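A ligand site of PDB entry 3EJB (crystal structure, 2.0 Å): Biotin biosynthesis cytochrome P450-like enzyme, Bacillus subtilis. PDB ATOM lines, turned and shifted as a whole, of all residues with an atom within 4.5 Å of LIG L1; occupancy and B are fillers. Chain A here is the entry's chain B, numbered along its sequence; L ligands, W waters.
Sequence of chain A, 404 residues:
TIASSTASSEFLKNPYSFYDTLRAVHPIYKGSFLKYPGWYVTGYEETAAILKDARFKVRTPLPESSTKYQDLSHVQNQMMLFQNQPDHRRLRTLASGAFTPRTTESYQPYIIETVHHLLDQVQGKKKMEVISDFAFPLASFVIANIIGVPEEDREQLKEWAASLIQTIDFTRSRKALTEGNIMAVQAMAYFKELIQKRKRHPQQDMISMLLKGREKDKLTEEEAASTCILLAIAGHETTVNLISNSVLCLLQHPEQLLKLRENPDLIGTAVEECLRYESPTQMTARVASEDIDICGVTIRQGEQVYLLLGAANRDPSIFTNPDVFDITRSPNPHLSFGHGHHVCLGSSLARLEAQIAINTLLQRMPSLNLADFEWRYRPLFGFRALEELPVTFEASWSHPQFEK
O1 of LIG L1 is in salt-bridge range of NH1 of Arg 92 (2.8 Å).
The side-chain hydroxyl (OG1) of Thr 284 sits at hydrogen-bond distance from an oxygen (O3) of LIG L1 (2.5 Å).
The side-chain sulfur of Cys 344 binds an iron atom (FE1) of LIG L1, at 2.4 Å.
NE2 of His 88 is in hydrogen-bond range of O1 of LIG L1, at 2.6 Å.
NH2 of Arg 286 lies within salt-bridge range of O4 of LIG L1.
ND1 of His 342 is in hydrogen-bond range of O2 of LIG L1 (2.8 Å).
The guanidinium group (NH1) of Arg 92 lies within hydrogen-bond range of the backbone carbonyl oxygen (O) of Val 343 (2.8 Å).
The backbone carbonyl oxygen (O) of Ala 234 sits at hydrogen-bond distance from the side-chain hydroxyl (OG1) of Thr 238.
The side-chain sulfur (SG) of Cys 344 lies close to the backbone NH (N) of Gly 346, at 3.4 Å.
The side-chain hydroxyl of Ser 336 lies within hydrogen-bond range of the backbone carbonyl oxygen of Leu 275, 2.6 Å away.
A ring nitrogen (NE2) of His 88 sits at hydrogen-bond distance from a ring nitrogen (ND1) of His 342 (3.4 Å).
N of Cys 344 lies within hydrogen-bond range of O of Phe 337 (3.0 Å).
The guanidinium group of Arg 286 lies within hydrogen-bond range of the side-chain hydroxyl of Thr 284 (3.5 Å).
Residues that only touch LIG L1: Met 80 (3.6 Å), Leu 81 (3.4 Å), Phe 99 (3.7 Å), Leu 230 (3.7 Å), Leu 231 (3.8 Å), Ala 234 (3.5 Å), Gly 235 (3.3 Å), Thr 238 (3.4 Å), Thr 239 (3.3 Å), Leu 275 (3.6 Å), Pro 280 (3.7 Å), Thr 281 (3.7 Å), Leu 309 (3.7 Å), Ser 336 (3.3 Å), Phe 337 (3.5 Å), Gly 338 (3.5 Å), His 341 (3.8 Å), Leu 345 (3.7 Å), Gly 346 (3.8 Å), Leu 349 (3.8 Å) and Ala 350 (3.9 Å).
Hydrophobic or aromatic side chains within 4 Å of LIG L1: Met 80, Leu 81, His 88, Phe 99, Leu 230, Leu 231, Ala 234, Leu 275, Pro 280, Leu 309, Phe 337, His 342, Leu 345, Leu 349 and Ala 350.
27 residues have an atom within 4 Å of LIG L1: Met 80, Leu 81, His 88, Arg 92, Phe 99, Leu 230, Leu 231, Ala 234, Gly 235, Thr 238, Thr 239, Leu 275, Pro 280, Thr 281, Thr 284, Arg 286, Leu 309, Ser 336, Phe 337, Gly 338, His 341, His 342, Cys 344, Leu 345, Gly 346, Leu 349 and Ala 350.
Water W2 lies within hydrogen-bond range of the backbone carbonyl oxygen (O) of Leu 81 (2.8 Å) and an oxygen (O3) of LIG L1 (2.9 Å).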
ATOM      1  N   MET A  80      10.405  10.579 -14.834  1.00  0.00           N
ATOM      2  CA  MET A  80      10.396   9.367 -15.656  1.00  0.00           C
ATOM      3  C   MET A  80       9.943   9.622 -17.089  1.00  0.00           C
ATOM      4  O   MET A  80      10.337   8.916 -18.015  1.00  0.00           O
ATOM      5  CB  MET A  80       9.508   8.300 -15.015  1.00  0.00           C
ATOM      6  CG  MET A  80       8.015   8.548 -15.175  1.00  0.00           C
ATOM      7  SD  MET A  80       6.984   7.219 -14.522  1.00  0.00           S
ATOM      8  CE  MET A  80       6.977   7.628 -12.782  1.00  0.00           C
ATOM      9  N   LEU A  81       9.113  10.647 -17.270  1.00  0.00           N
ATOM     10  CA  LEU A  81       8.571  11.017 -18.567  1.00  0.00           C
ATOM     11  C   LEU A  81       9.677  11.377 -19.560  1.00  0.00           C
ATOM     12  O   LEU A  81       9.515  11.221 -20.777  1.00  0.00           O
ATOM     13  CB  LEU A  81       7.587  12.189 -18.420  1.00  0.00           C
ATOM     14  CG  LEU A  81       6.837  12.709 -19.644  1.00  0.00           C
ATOM     15  CD1 LEU A  81       5.958  11.624 -20.254  1.00  0.00           C
ATOM     16  CD2 LEU A  81       5.995  13.918 -19.258  1.00  0.00           C
ATOM     17  N   HIS A  88      14.427   4.905 -16.631  1.00  0.00           N
ATOM     18  CA  HIS A  88      12.975   4.981 -16.801  1.00  0.00           C
ATOM     19  C   HIS A  88      12.241   3.838 -16.088  1.00  0.00           C
ATOM     20  O   HIS A  88      11.291   4.077 -15.351  1.00  0.00           O
ATOM     21  CB  HIS A  88      12.581   4.995 -18.273  1.00  0.00           C
ATOM     22  CG  HIS A  88      11.121   4.765 -18.507  1.00  0.00           C
ATOM     23  ND1 HIS A  88      10.625   3.664 -19.172  1.00  0.00           N
ATOM     24  CD2 HIS A  88      10.040   5.492 -18.131  1.00  0.00           C
ATOM     25  CE1 HIS A  88       9.312   3.722 -19.206  1.00  0.00           C
ATOM     26  NE2 HIS A  88       8.932   4.822 -18.582  1.00  0.00           N
ATOM     27  N   ARG A  92       9.590   4.259 -13.056  1.00  0.00           N
ATOM     28  CA  ARG A  92       8.205   3.912 -13.332  1.00  0.00           C
ATOM     29  C   ARG A  92       7.708   2.809 -12.406  1.00  0.00           C
ATOM     30  O   ARG A  92       6.628   2.912 -11.822  1.00  0.00           O
ATOM     31  CB  ARG A  92       8.021   3.503 -14.800  1.00  0.00           C
ATOM     32  CG  ARG A  92       6.568   3.253 -15.199  1.00  0.00           C
ATOM     33  CD  ARG A  92       6.447   2.805 -16.640  1.00  0.00           C
ATOM     34  NE  ARG A  92       5.109   2.277 -16.934  1.00  0.00           N
ATOM     35  CZ  ARG A  92       4.161   2.968 -17.551  1.00  0.00           C
ATOM     36  NH1 ARG A  92       4.380   4.207 -17.953  1.00  0.00           N
ATOM     37  NH2 ARG A  92       2.977   2.405 -17.770  1.00  0.00           N
ATOM     38  N   PHE A  99      -0.969   2.839  -8.712  1.00  0.00           N
ATOM     39  CA  PHE A  99      -1.827   2.945  -9.892  1.00  0.00           C
ATOM     40  C   PHE A  99      -2.174   1.603 -10.535  1.00  0.00           C
ATOM     41  O   PHE A  99      -2.603   1.548 -11.692  1.00  0.00           O
ATOM     42  CB  PHE A  99      -1.195   3.879 -10.933  1.00  0.00           C
ATOM     43  CG  PHE A  99      -0.939   5.263 -10.428  1.00  0.00           C
ATOM     44  CD1 PHE A  99      -1.956   6.205 -10.417  1.00  0.00           C
ATOM     45  CD2 PHE A  99       0.310   5.616  -9.939  1.00  0.00           C
ATOM     46  CE1 PHE A  99      -1.725   7.484  -9.935  1.00  0.00           C
ATOM     47  CE2 PHE A  99       0.549   6.896  -9.463  1.00  0.00           C
ATOM     48  CZ  PHE A  99      -0.476   7.830  -9.461  1.00  0.00           C
ATOM     49  N   ILE A 143      -5.931  13.412  -6.450  1.00  0.00           N
ATOM     50  CA  ILE A 143      -4.489  13.204  -6.602  1.00  0.00           C
ATOM     51  C   ILE A 143      -3.718  13.628  -5.349  1.00  0.00           C
ATOM     52  O   ILE A 143      -2.755  12.976  -4.964  1.00  0.00           O
ATOM     53  CB  ILE A 143      -3.927  13.914  -7.855  1.00  0.00           C
ATOM     54  CG1 ILE A 143      -2.559  13.339  -8.232  1.00  0.00           C
ATOM     55  CG2 ILE A 143      -3.845  15.419  -7.648  1.00  0.00           C
ATOM     56  CD1 ILE A 143      -2.571  11.845  -8.480  1.00  0.00           C
ATOM     57  N   LEU A 230       5.522  15.438 -10.862  1.00  0.00           N
ATOM     58  CA  LEU A 230       4.999  14.911 -12.120  1.00  0.00           C
ATOM     59  C   LEU A 230       3.556  14.448 -11.969  1.00  0.00           C
ATOM     60  O   LEU A 230       2.685  14.819 -12.768  1.00  0.00           O
ATOM     61  CB  LEU A 230       5.873  13.759 -12.619  1.00  0.00           C
ATOM     62  CG  LEU A 230       5.367  12.979 -13.843  1.00  0.00           C
ATOM     63  CD1 LEU A 230       5.158  13.906 -15.042  1.00  0.00           C
ATOM     64  CD2 LEU A 230       6.307  11.850 -14.198  1.00  0.00           C
ATOM     65  N   LEU A 231       3.303  13.644 -10.947  1.00  0.00           N
ATOM     66  CA  LEU A 231       1.966  13.080 -10.722  1.00  0.00           C
ATOM     67  C   LEU A 231       0.956  14.152 -10.346  1.00  0.00           C
ATOM     68  O   LEU A 231      -0.201  14.091 -10.766  1.00  0.00           O
ATOM     69  CB  LEU A 231       2.031  11.990  -9.647  1.00  0.00           C
ATOM     70  CG  LEU A 231       2.845  10.757 -10.006  1.00  0.00           C
ATOM     71  CD1 LEU A 231       3.102   9.907  -8.775  1.00  0.00           C
ATOM     72  CD2 LEU A 231       2.162   9.935 -11.085  1.00  0.00           C
ATOM     73  N   ALA A 234       0.048  16.003 -13.703  1.00  0.00           N
ATOM     74  CA  ALA A 234      -0.813  15.166 -14.542  1.00  0.00           C
ATOM     75  C   ALA A 234      -2.227  15.055 -13.969  1.00  0.00           C
ATOM     76  O   ALA A 234      -3.219  15.072 -14.702  1.00  0.00           O
ATOM     77  CB  ALA A 234      -0.208  13.798 -14.738  1.00  0.00           C
ATOM     78  N   GLY A 235      -2.316  14.942 -12.650  1.00  0.00           N
ATOM     79  CA  GLY A 235      -3.599  14.842 -11.964  1.00  0.00           C
ATOM     80  C   GLY A 235      -4.434  16.112 -12.039  1.00  0.00           C
ATOM     81  O   GLY A 235      -5.659  16.056 -11.974  1.00  0.00           O
ATOM     82  N   THR A 238      -4.664  17.105 -17.091  1.00  0.00           N
ATOM     83  CA  THR A 238      -5.232  16.253 -18.127  1.00  0.00           C
ATOM     84  C   THR A 238      -6.588  15.648 -17.739  1.00  0.00           C
ATOM     85  O   THR A 238      -7.513  15.602 -18.554  1.00  0.00           O
ATOM     86  CB  THR A 238      -4.267  15.122 -18.530  1.00  0.00           C
ATOM     87  OG1 THR A 238      -3.575  14.658 -17.358  1.00  0.00           O
ATOM     88  CG2 THR A 238      -3.256  15.621 -19.551  1.00  0.00           C
ATOM     89  N   THR A 239      -6.700  15.183 -16.504  1.00  0.00           N
ATOM     90  CA  THR A 239      -7.927  14.563 -16.024  1.00  0.00           C
ATOM     91  C   THR A 239      -9.091  15.558 -16.045  1.00  0.00           C
ATOM     92  O   THR A 239     -10.218  15.212 -16.402  1.00  0.00           O
ATOM     93  CB  THR A 239      -7.771  13.975 -14.614  1.00  0.00           C
ATOM     94  OG1 THR A 239      -6.585  13.157 -14.567  1.00  0.00           O
ATOM     95  CG2 THR A 239      -8.969  13.126 -14.240  1.00  0.00           C
ATOM     96  N   LEU A 242     -10.235  15.859 -19.579  1.00  0.00           N
ATOM     97  CA  LEU A 242     -10.997  14.672 -19.960  1.00  0.00           C
ATOM     98  C   LEU A 242     -12.469  14.808 -19.566  1.00  0.00           C
ATOM     99  O   LEU A 242     -13.364  14.577 -20.372  1.00  0.00           O
ATOM    100  CB  LEU A 242     -10.392  13.413 -19.328  1.00  0.00           C
ATOM    101  CG  LEU A 242     -11.207  12.124 -19.418  1.00  0.00           C
ATOM    102  CD1 LEU A 242     -11.502  11.747 -20.861  1.00  0.00           C
ATOM    103  CD2 LEU A 242     -10.469  10.991 -18.710  1.00  0.00           C
ATOM    104  N   LEU A 275     -12.427  10.081 -25.322  1.00  0.00           N
ATOM    105  CA  LEU A 275     -10.970  10.113 -25.360  1.00  0.00           C
ATOM    106  C   LEU A 275     -10.446  10.197 -26.798  1.00  0.00           C
ATOM    107  O   LEU A 275      -9.494  10.922 -27.070  1.00  0.00           O
ATOM    108  CB  LEU A 275     -10.402   8.874 -24.662  1.00  0.00           C
ATOM    109  CG  LEU A 275     -10.292   8.944 -23.134  1.00  0.00           C
ATOM    110  CD1 LEU A 275     -10.278   7.558 -22.522  1.00  0.00           C
ATOM    111  CD2 LEU A 275      -9.042   9.738 -22.724  1.00  0.00           C
ATOM    112  N   PRO A 280      -7.431  14.854 -24.532  1.00  0.00           N
ATOM    113  CA  PRO A 280      -6.894  15.845 -23.603  1.00  0.00           C
ATOM    114  C   PRO A 280      -5.450  16.216 -23.916  1.00  0.00           C
ATOM    115  O   PRO A 280      -5.059  17.375 -23.783  1.00  0.00           O
ATOM    116  CB  PRO A 280      -6.975  15.124 -22.253  1.00  0.00           C
ATOM    117  CG  PRO A 280      -8.073  14.143 -22.415  1.00  0.00           C
ATOM    118  CD  PRO A 280      -7.948  13.671 -23.841  1.00  0.00           C
ATOM    119  N   THR A 281      -4.660  15.223 -24.333  1.00  0.00           N
ATOM    120  CA  THR A 281      -3.276  15.464 -24.745  1.00  0.00           C
ATOM    121  C   THR A 281      -3.151  15.350 -26.256  1.00  0.00           C
ATOM    122  O   THR A 281      -3.407  14.290 -26.833  1.00  0.00           O
ATOM    123  CB  THR A 281      -2.310  14.462 -24.080  1.00  0.00           C
ATOM    124  OG1 THR A 281      -2.403  14.562 -22.656  1.00  0.00           O
ATOM    125  CG2 THR A 281      -0.869  14.730 -24.515  1.00  0.00           C
ATOM    126  N   THR A 284       2.788  14.463 -28.031  1.00  0.00           N
ATOM    127  CA  THR A 284       4.025  14.122 -27.337  1.00  0.00           C
ATOM    128  C   THR A 284       5.171  14.136 -28.354  1.00  0.00           C
ATOM    129  O   THR A 284       4.947  14.360 -29.541  1.00  0.00           O
ATOM    130  CB  THR A 284       3.937  12.774 -26.609  1.00  0.00           C
ATOM    131  OG1 THR A 284       5.039  12.639 -25.702  1.00  0.00           O
ATOM    132  CG2 THR A 284       3.943  11.615 -27.599  1.00  0.00           C
ATOM    133  N   ARG A 286       9.418  12.806 -29.554  1.00  0.00           N
ATOM    134  CA  ARG A 286      10.575  11.920 -29.469  1.00  0.00           C
ATOM    135  C   ARG A 286      11.740  12.511 -30.265  1.00  0.00           C
ATOM    136  O   ARG A 286      11.549  13.339 -31.149  1.00  0.00           O
ATOM    137  CB  ARG A 286      10.226  10.523 -30.024  1.00  0.00           C
ATOM    138  CG  ARG A 286       9.149   9.775 -29.244  1.00  0.00           C
ATOM    139  CD  ARG A 286       9.655   9.349 -27.870  1.00  0.00           C
ATOM    140  NE  ARG A 286       8.712   8.476 -27.172  1.00  0.00           N
ATOM    141  CZ  ARG A 286       7.682   8.902 -26.455  1.00  0.00           C
ATOM    142  NH1 ARG A 286       7.438  10.203 -26.345  1.00  0.00           N
ATOM    143  NH2 ARG A 286       6.896   8.034 -25.833  1.00  0.00           N
ATOM    144  N   LEU A 309      -1.452  13.126 -31.380  1.00  0.00           N
ATOM    145  CA  LEU A 309      -2.303  12.033 -30.932  1.00  0.00           C
ATOM    146  C   LEU A 309      -3.759  12.242 -31.318  1.00  0.00           C
ATOM    147  O   LEU A 309      -4.463  11.301 -31.674  1.00  0.00           O
ATOM    148  CB  LEU A 309      -2.188  11.853 -29.416  1.00  0.00           C
ATOM    149  CG  LEU A 309      -0.788  11.645 -28.846  1.00  0.00           C
ATOM    150  CD1 LEU A 309      -0.833  11.607 -27.327  1.00  0.00           C
ATOM    151  CD2 LEU A 309      -0.156  10.368 -29.398  1.00  0.00           C
ATOM    152  N   SER A 336      -4.815   8.067 -27.095  1.00  0.00           N
ATOM    153  CA  SER A 336      -4.910   9.242 -26.228  1.00  0.00           C
ATOM    154  C   SER A 336      -4.007   9.125 -24.995  1.00  0.00           C
ATOM    155  O   SER A 336      -3.571  10.130 -24.441  1.00  0.00           O
ATOM    156  CB  SER A 336      -6.355   9.493 -25.809  1.00  0.00           C
ATOM    157  OG  SER A 336      -7.140   9.864 -26.928  1.00  0.00           O
ATOM    158  N   PHE A 337      -3.744   7.886 -24.574  1.00  0.00           N
ATOM    159  CA  PHE A 337      -2.852   7.630 -23.442  1.00  0.00           C
ATOM    160  C   PHE A 337      -1.459   7.235 -23.918  1.00  0.00           C
ATOM    161  O   PHE A 337      -0.638   6.779 -23.125  1.00  0.00           O
ATOM    162  CB  PHE A 337      -3.431   6.539 -22.552  1.00  0.00           C
ATOM    163  CG  PHE A 337      -4.618   6.972 -21.727  1.00  0.00           C
ATOM    164  CD1 PHE A 337      -5.866   6.416 -21.931  1.00  0.00           C
ATOM    165  CD2 PHE A 337      -4.470   7.942 -20.753  1.00  0.00           C
ATOM    166  CE1 PHE A 337      -6.953   6.820 -21.175  1.00  0.00           C
ATOM    167  CE2 PHE A 337      -5.549   8.353 -19.987  1.00  0.00           C
ATOM    168  CZ  PHE A 337      -6.798   7.790 -20.207  1.00  0.00           C
ATOM    169  N   GLY A 338      -1.201   7.416 -25.201  1.00  0.00           N
ATOM    170  CA  GLY A 338       0.093   7.066 -25.780  1.00  0.00           C
ATOM    171  C   GLY A 338       0.182   5.587 -26.107  1.00  0.00           C
ATOM    172  O   GLY A 338      -0.834   4.920 -26.319  1.00  0.00           O
ATOM    173  N   HIS A 341       6.405   1.926 -23.993  1.00  0.00           N
ATOM    174  CA  HIS A 341       6.973   1.874 -22.642  1.00  0.00           C
ATOM    175  C   HIS A 341       6.515   3.014 -21.731  1.00  0.00           C
ATOM    176  O   HIS A 341       6.440   2.861 -20.509  1.00  0.00           O
ATOM    177  CB  HIS A 341       8.493   1.849 -22.702  1.00  0.00           C
ATOM    178  CG  HIS A 341       9.060   0.595 -23.299  1.00  0.00           C
ATOM    179  ND1 HIS A 341       8.611  -0.662 -22.957  1.00  0.00           N
ATOM    180  CD2 HIS A 341      10.052   0.404 -24.202  1.00  0.00           C
ATOM    181  CE1 HIS A 341       9.290  -1.567 -23.629  1.00  0.00           C
ATOM    182  NE2 HIS A 341      10.169  -0.949 -24.392  1.00  0.00           N
ATOM    183  N   HIS A 342       6.230   4.178 -22.328  1.00  0.00           N
ATOM    184  CA  HIS A 342       5.861   5.362 -21.557  1.00  0.00           C
ATOM    185  C   HIS A 342       4.345   5.542 -21.450  1.00  0.00           C
ATOM    186  O   HIS A 342       3.867   6.570 -20.966  1.00  0.00           O
ATOM    187  CB  HIS A 342       6.494   6.619 -22.164  1.00  0.00           C
ATOM    188  CG  HIS A 342       7.974   6.702 -21.981  1.00  0.00           C
ATOM    189  ND1 HIS A 342       8.556   7.259 -20.870  1.00  0.00           N
ATOM    190  CD2 HIS A 342       9.001   6.309 -22.777  1.00  0.00           C
ATOM    191  CE1 HIS A 342       9.872   7.206 -20.975  1.00  0.00           C
ATOM    192  NE2 HIS A 342      10.162   6.633 -22.129  1.00  0.00           N
ATOM    193  N   VAL A 343       3.600   4.536 -21.893  1.00  0.00           N
ATOM    194  CA  VAL A 343       2.134   4.606 -21.875  1.00  0.00           C
ATOM    195  C   VAL A 343       1.606   5.058 -20.515  1.00  0.00           C
ATOM    196  O   VAL A 343       2.096   4.621 -19.476  1.00  0.00           O
ATOM    197  CB  VAL A 343       1.488   3.250 -22.285  1.00  0.00           C
ATOM    198  CG1 VAL A 343       1.598   2.231 -21.150  1.00  0.00           C
ATOM    199  CG2 VAL A 343       0.040   3.447 -22.709  1.00  0.00           C
ATOM    200  N   CYS A 344       0.627   5.960 -20.538  1.00  0.00           N
ATOM    201  CA  CYS A 344       0.154   6.619 -19.317  1.00  0.00           C
ATOM    202  C   CYS A 344       0.104   5.699 -18.103  1.00  0.00           C
ATOM    203  O   CYS A 344      -0.514   4.637 -18.142  1.00  0.00           O
ATOM    204  CB  CYS A 344      -1.228   7.247 -19.551  1.00  0.00           C
ATOM    205  SG  CYS A 344      -1.857   8.159 -18.123  1.00  0.00           S
ATOM    206  N   LEU A 345       0.757   6.127 -17.024  1.00  0.00           N
ATOM    207  CA  LEU A 345       0.789   5.346 -15.794  1.00  0.00           C
ATOM    208  C   LEU A 345      -0.553   5.416 -15.043  1.00  0.00           C
ATOM    209  O   LEU A 345      -0.918   4.477 -14.339  1.00  0.00           O
ATOM    210  CB  LEU A 345       1.920   5.836 -14.887  1.00  0.00           C
ATOM    211  CG  LEU A 345       2.270   4.975 -13.671  1.00  0.00           C
ATOM    212  CD1 LEU A 345       2.753   3.598 -14.111  1.00  0.00           C
ATOM    213  CD2 LEU A 345       3.310   5.661 -12.813  1.00  0.00           C
ATOM    214  N   GLY A 346      -1.269   6.523 -15.204  1.00  0.00           N
ATOM    215  CA  GLY A 346      -2.481   6.763 -14.424  1.00  0.00           C
ATOM    216  C   GLY A 346      -3.777   6.634 -15.207  1.00  0.00           C
ATOM    217  O   GLY A 346      -4.809   7.166 -14.801  1.00  0.00           O
ATOM    218  N   LEU A 349      -6.861   5.378 -13.310  1.00  0.00           N
ATOM    219  CA  LEU A 349      -7.369   6.402 -12.404  1.00  0.00           C
ATOM    220  C   LEU A 349      -8.175   7.457 -13.169  1.00  0.00           C
ATOM    221  O   LEU A 349      -9.274   7.828 -12.746  1.00  0.00           O
ATOM    222  CB  LEU A 349      -6.228   7.052 -11.632  1.00  0.00           C
ATOM    223  CG  LEU A 349      -6.570   8.235 -10.718  1.00  0.00           C
ATOM    224  CD1 LEU A 349      -7.512   7.801  -9.593  1.00  0.00           C
ATOM    225  CD2 LEU A 349      -5.312   8.860 -10.152  1.00  0.00           C
ATOM    226  N   ALA A 350      -7.632   7.913 -14.290  1.00  0.00           N
ATOM    227  CA  ALA A 350      -8.284   8.926 -15.107  1.00  0.00           C
ATOM    228  C   ALA A 350      -9.636   8.432 -15.636  1.00  0.00           C
ATOM    229  O   ALA A 350     -10.614   9.183 -15.639  1.00  0.00           O
ATOM    230  CB  ALA A 350      -7.393   9.345 -16.264  1.00  0.00           C
ATOM    231  N   GLU A 353     -12.155   8.248 -12.581  1.00  0.00           N
ATOM    232  CA  GLU A 353     -12.596   9.587 -12.220  1.00  0.00           C
ATOM    233  C   GLU A 353     -13.635  10.113 -13.211  1.00  0.00           C
ATOM    234  O   GLU A 353     -14.657  10.665 -12.807  1.00  0.00           O
ATOM    235  CB  GLU A 353     -11.400  10.555 -12.146  1.00  0.00           C
ATOM    236  CG  GLU A 353     -10.514  10.380 -10.921  1.00  0.00           C
ATOM    237  CD  GLU A 353      -9.532  11.520 -10.733  1.00  0.00           C
ATOM    238  OE1 GLU A 353      -9.979  12.665 -10.502  1.00  0.00           O
ATOM    239  OE2 GLU A 353      -8.309  11.286 -10.806  1.00  0.00           O
HETATM  240  C1  LIG L   1       2.276   9.453 -19.450  1.00  0.00           C
HETATM  241  C2  LIG L   1       0.518  10.057 -14.970  1.00  0.00           C
HETATM  242  C3  LIG L   1      -3.833  11.224 -16.811  1.00  0.00           C
HETATM  243  C4  LIG L   1      -1.939  11.165 -21.291  1.00  0.00           C
HETATM  244  C5  LIG L   1       2.191   9.536 -18.081  1.00  0.00           C
HETATM  245  C6  LIG L   1       3.270   9.323 -17.145  1.00  0.00           C
HETATM  246  C7  LIG L   1       2.782   9.478 -15.914  1.00  0.00           C
HETATM  247  C8  LIG L   1       1.381   9.812 -16.020  1.00  0.00           C
HETATM  248  C9  LIG L   1       3.591   9.352 -14.591  1.00  0.00           C
HETATM  249  C10 LIG L   1       4.735   8.962 -17.516  1.00  0.00           C
HETATM  250  C11 LIG L   1       4.862   7.447 -17.658  1.00  0.00           C
HETATM  251  C12 LIG L   1       6.222   7.083 -18.188  1.00  0.00           C
HETATM  252  O1  LIG L   1       6.582   5.886 -18.134  1.00  0.00           O
HETATM  253  O2  LIG L   1       6.948   7.988 -18.676  1.00  0.00           O
HETATM  254  C13 LIG L   1      -0.831  10.362 -15.077  1.00  0.00           C
HETATM  255  C14 LIG L   1      -1.772  10.429 -13.980  1.00  0.00           C
HETATM  256  C15 LIG L   1      -2.970  10.743 -14.485  1.00  0.00           C
HETATM  257  C16 LIG L   1      -2.824  10.889 -15.921  1.00  0.00           C
HETATM  258  C17 LIG L   1      -1.424  10.168 -12.501  1.00  0.00           C
HETATM  259  C18 LIG L   1      -4.288  10.924 -13.695  1.00  0.00           C
HETATM  260  C19 LIG L   1      -4.318  11.643 -12.577  1.00  0.00           C
HETATM  261  C20 LIG L   1      -3.707  11.324 -18.180  1.00  0.00           C
HETATM  262  C21 LIG L   1      -4.742  11.697 -19.114  1.00  0.00           C
HETATM  263  C22 LIG L   1      -4.223  11.673 -20.345  1.00  0.00           C
HETATM  264  C23 LIG L   1      -2.829  11.298 -20.236  1.00  0.00           C
HETATM  265  C24 LIG L   1      -6.200  12.050 -18.752  1.00  0.00           C
HETATM  266  C25 LIG L   1      -4.950  12.006 -21.665  1.00  0.00           C
HETATM  267  C26 LIG L   1      -5.796  11.128 -22.205  1.00  0.00           C
HETATM  268  C27 LIG L   1      -0.669  10.645 -21.233  1.00  0.00           C
HETATM  269  C28 LIG L   1       0.159  10.337 -22.375  1.00  0.00           C
HETATM  270  C29 LIG L   1       1.472   9.808 -21.808  1.00  0.00           C
HETATM  271  C30 LIG L   1       1.317   9.851 -20.369  1.00  0.00           C
HETATM  272  C31 LIG L   1      -0.210  10.520 -23.868  1.00  0.00           C
HETATM  273  C32 LIG L   1       2.705   9.325 -22.596  1.00  0.00           C
HETATM  274  C33 LIG L   1       3.577  10.514 -22.981  1.00  0.00           C
HETATM  275  C34 LIG L   1       4.742  10.041 -23.803  1.00  0.00           C
HETATM  276  O3  LIG L   1       5.641  10.865 -24.101  1.00  0.00           O
HETATM  277  O4  LIG L   1       4.770   8.845 -24.169  1.00  0.00           O
HETATM  278  N1  LIG L   1       1.043   9.833 -17.359  1.00  0.00           N
HETATM  279  N2  LIG L   1      -1.505  10.653 -16.241  1.00  0.00           N
HETATM  280  N3  LIG L   1      -2.548  11.087 -18.900  1.00  0.00           N
HETATM  281  N4  LIG L   1       0.047  10.346 -20.067  1.00  0.00           N
HETATM  282 FE1  LIG L   1      -0.806  10.294 -18.160  1.00  0.00          FE
HETATM  283  O1  LG2 L   2      19.129  21.038 -27.098  1.00  0.00           O
HETATM  284  P1  LG2 L   2      18.184  21.269 -28.454  1.00  0.00           P
HETATM  285  O2  LG2 L   2      18.736  20.674 -29.921  1.00  0.00           O
HETATM  286  O3  LG2 L   2      16.374  21.348 -28.223  1.00  0.00           O
HETATM  287  C1  LG2 L   2      15.626  20.133 -28.242  1.00  0.00           C
HETATM  288  C2  LG2 L   2      14.270  20.334 -27.576  1.00  0.00           C
HETATM  289  C3  LG2 L   2      14.396  21.418 -26.509  1.00  0.00           C
HETATM  290  C4  LG2 L   2      13.848  19.029 -26.920  1.00  0.00           C
HETATM  291  C5  LG2 L   2      13.241  20.690 -28.646  1.00  0.00           C
HETATM  292  O4  LG2 L   2      13.869  21.293 -29.779  1.00  0.00           O
HETATM  293  C6  LG2 L   2      12.130  21.575 -28.139  1.00  0.00           C
HETATM  294  O5  LG2 L   2      12.386  22.626 -27.374  1.00  0.00           O
HETATM  295  N1  LG2 L   2      10.941  21.295 -28.471  1.00  0.00           N
HETATM  296  C7  LG2 L   2       9.712  21.991 -28.120  1.00  0.00           C
HETATM  297  C8  LG2 L   2       9.351  21.531 -26.714  1.00  0.00           C
HETATM  298  C9  LG2 L   2       8.917  20.077 -26.699  1.00  0.00           C
HETATM  299  O6  LG2 L   2       9.436  19.209 -27.564  1.00  0.00           O
HETATM  300  N2  LG2 L   2       8.067  19.684 -25.854  1.00  0.00           N
HETATM  301  C10 LG2 L   2       7.562  18.335 -25.681  1.00  0.00           C
HETATM  302  C11 LG2 L   2       6.149  18.314 -26.252  1.00  0.00           C
HETATM  303  S1  LG2 L   2       5.100  17.280 -25.284  1.00  0.00           S
HETATM  304  C12 LG2 L   2       5.999  15.929 -24.569  1.00  0.00           C
HETATM  305  O7  LG2 L   2       7.225  15.668 -24.971  1.00  0.00           O
HETATM  306  C13 LG2 L   2       5.288  14.961 -23.625  1.00  0.00           C
HETATM  307  C14 LG2 L   2       4.192  15.646 -22.815  1.00  0.00           C
HETATM  308  C15 LG2 L   2       2.839  14.980 -23.057  1.00  0.00           C
HETATM  309  C16 LG2 L   2       2.556  13.897 -22.028  1.00  0.00           C
HETATM  310  C17 LG2 L   2       1.470  14.314 -21.049  1.00  0.00           C
HETATM  311  C18 LG2 L   2       1.683  13.666 -19.684  1.00  0.00           C
HETATM  312  C19 LG2 L   2       0.847  14.339 -18.604  1.00  0.00           C
HETATM  313  C20 LG2 L   2       1.353  15.751 -18.314  1.00  0.00           C
HETATM  314  C21 LG2 L   2       2.619  15.960 -17.499  1.00  0.00           C
HETATM  315  C22 LG2 L   2       3.523  17.161 -17.796  1.00  0.00           C
HETATM  316  C23 LG2 L   2       4.703  17.232 -16.843  1.00  0.00           C
HETATM  317  C24 LG2 L   2       5.724  18.254 -17.326  1.00  0.00           C
HETATM  318  C25 LG2 L   2       6.521  18.833 -16.156  1.00  0.00           C
HETATM  319  O   HOH W   1       3.434   6.594 -24.804  1.00  0.00           O
HETATM  320  O   HOH W   2       7.960  12.143 -22.953  1.00  0.00           O
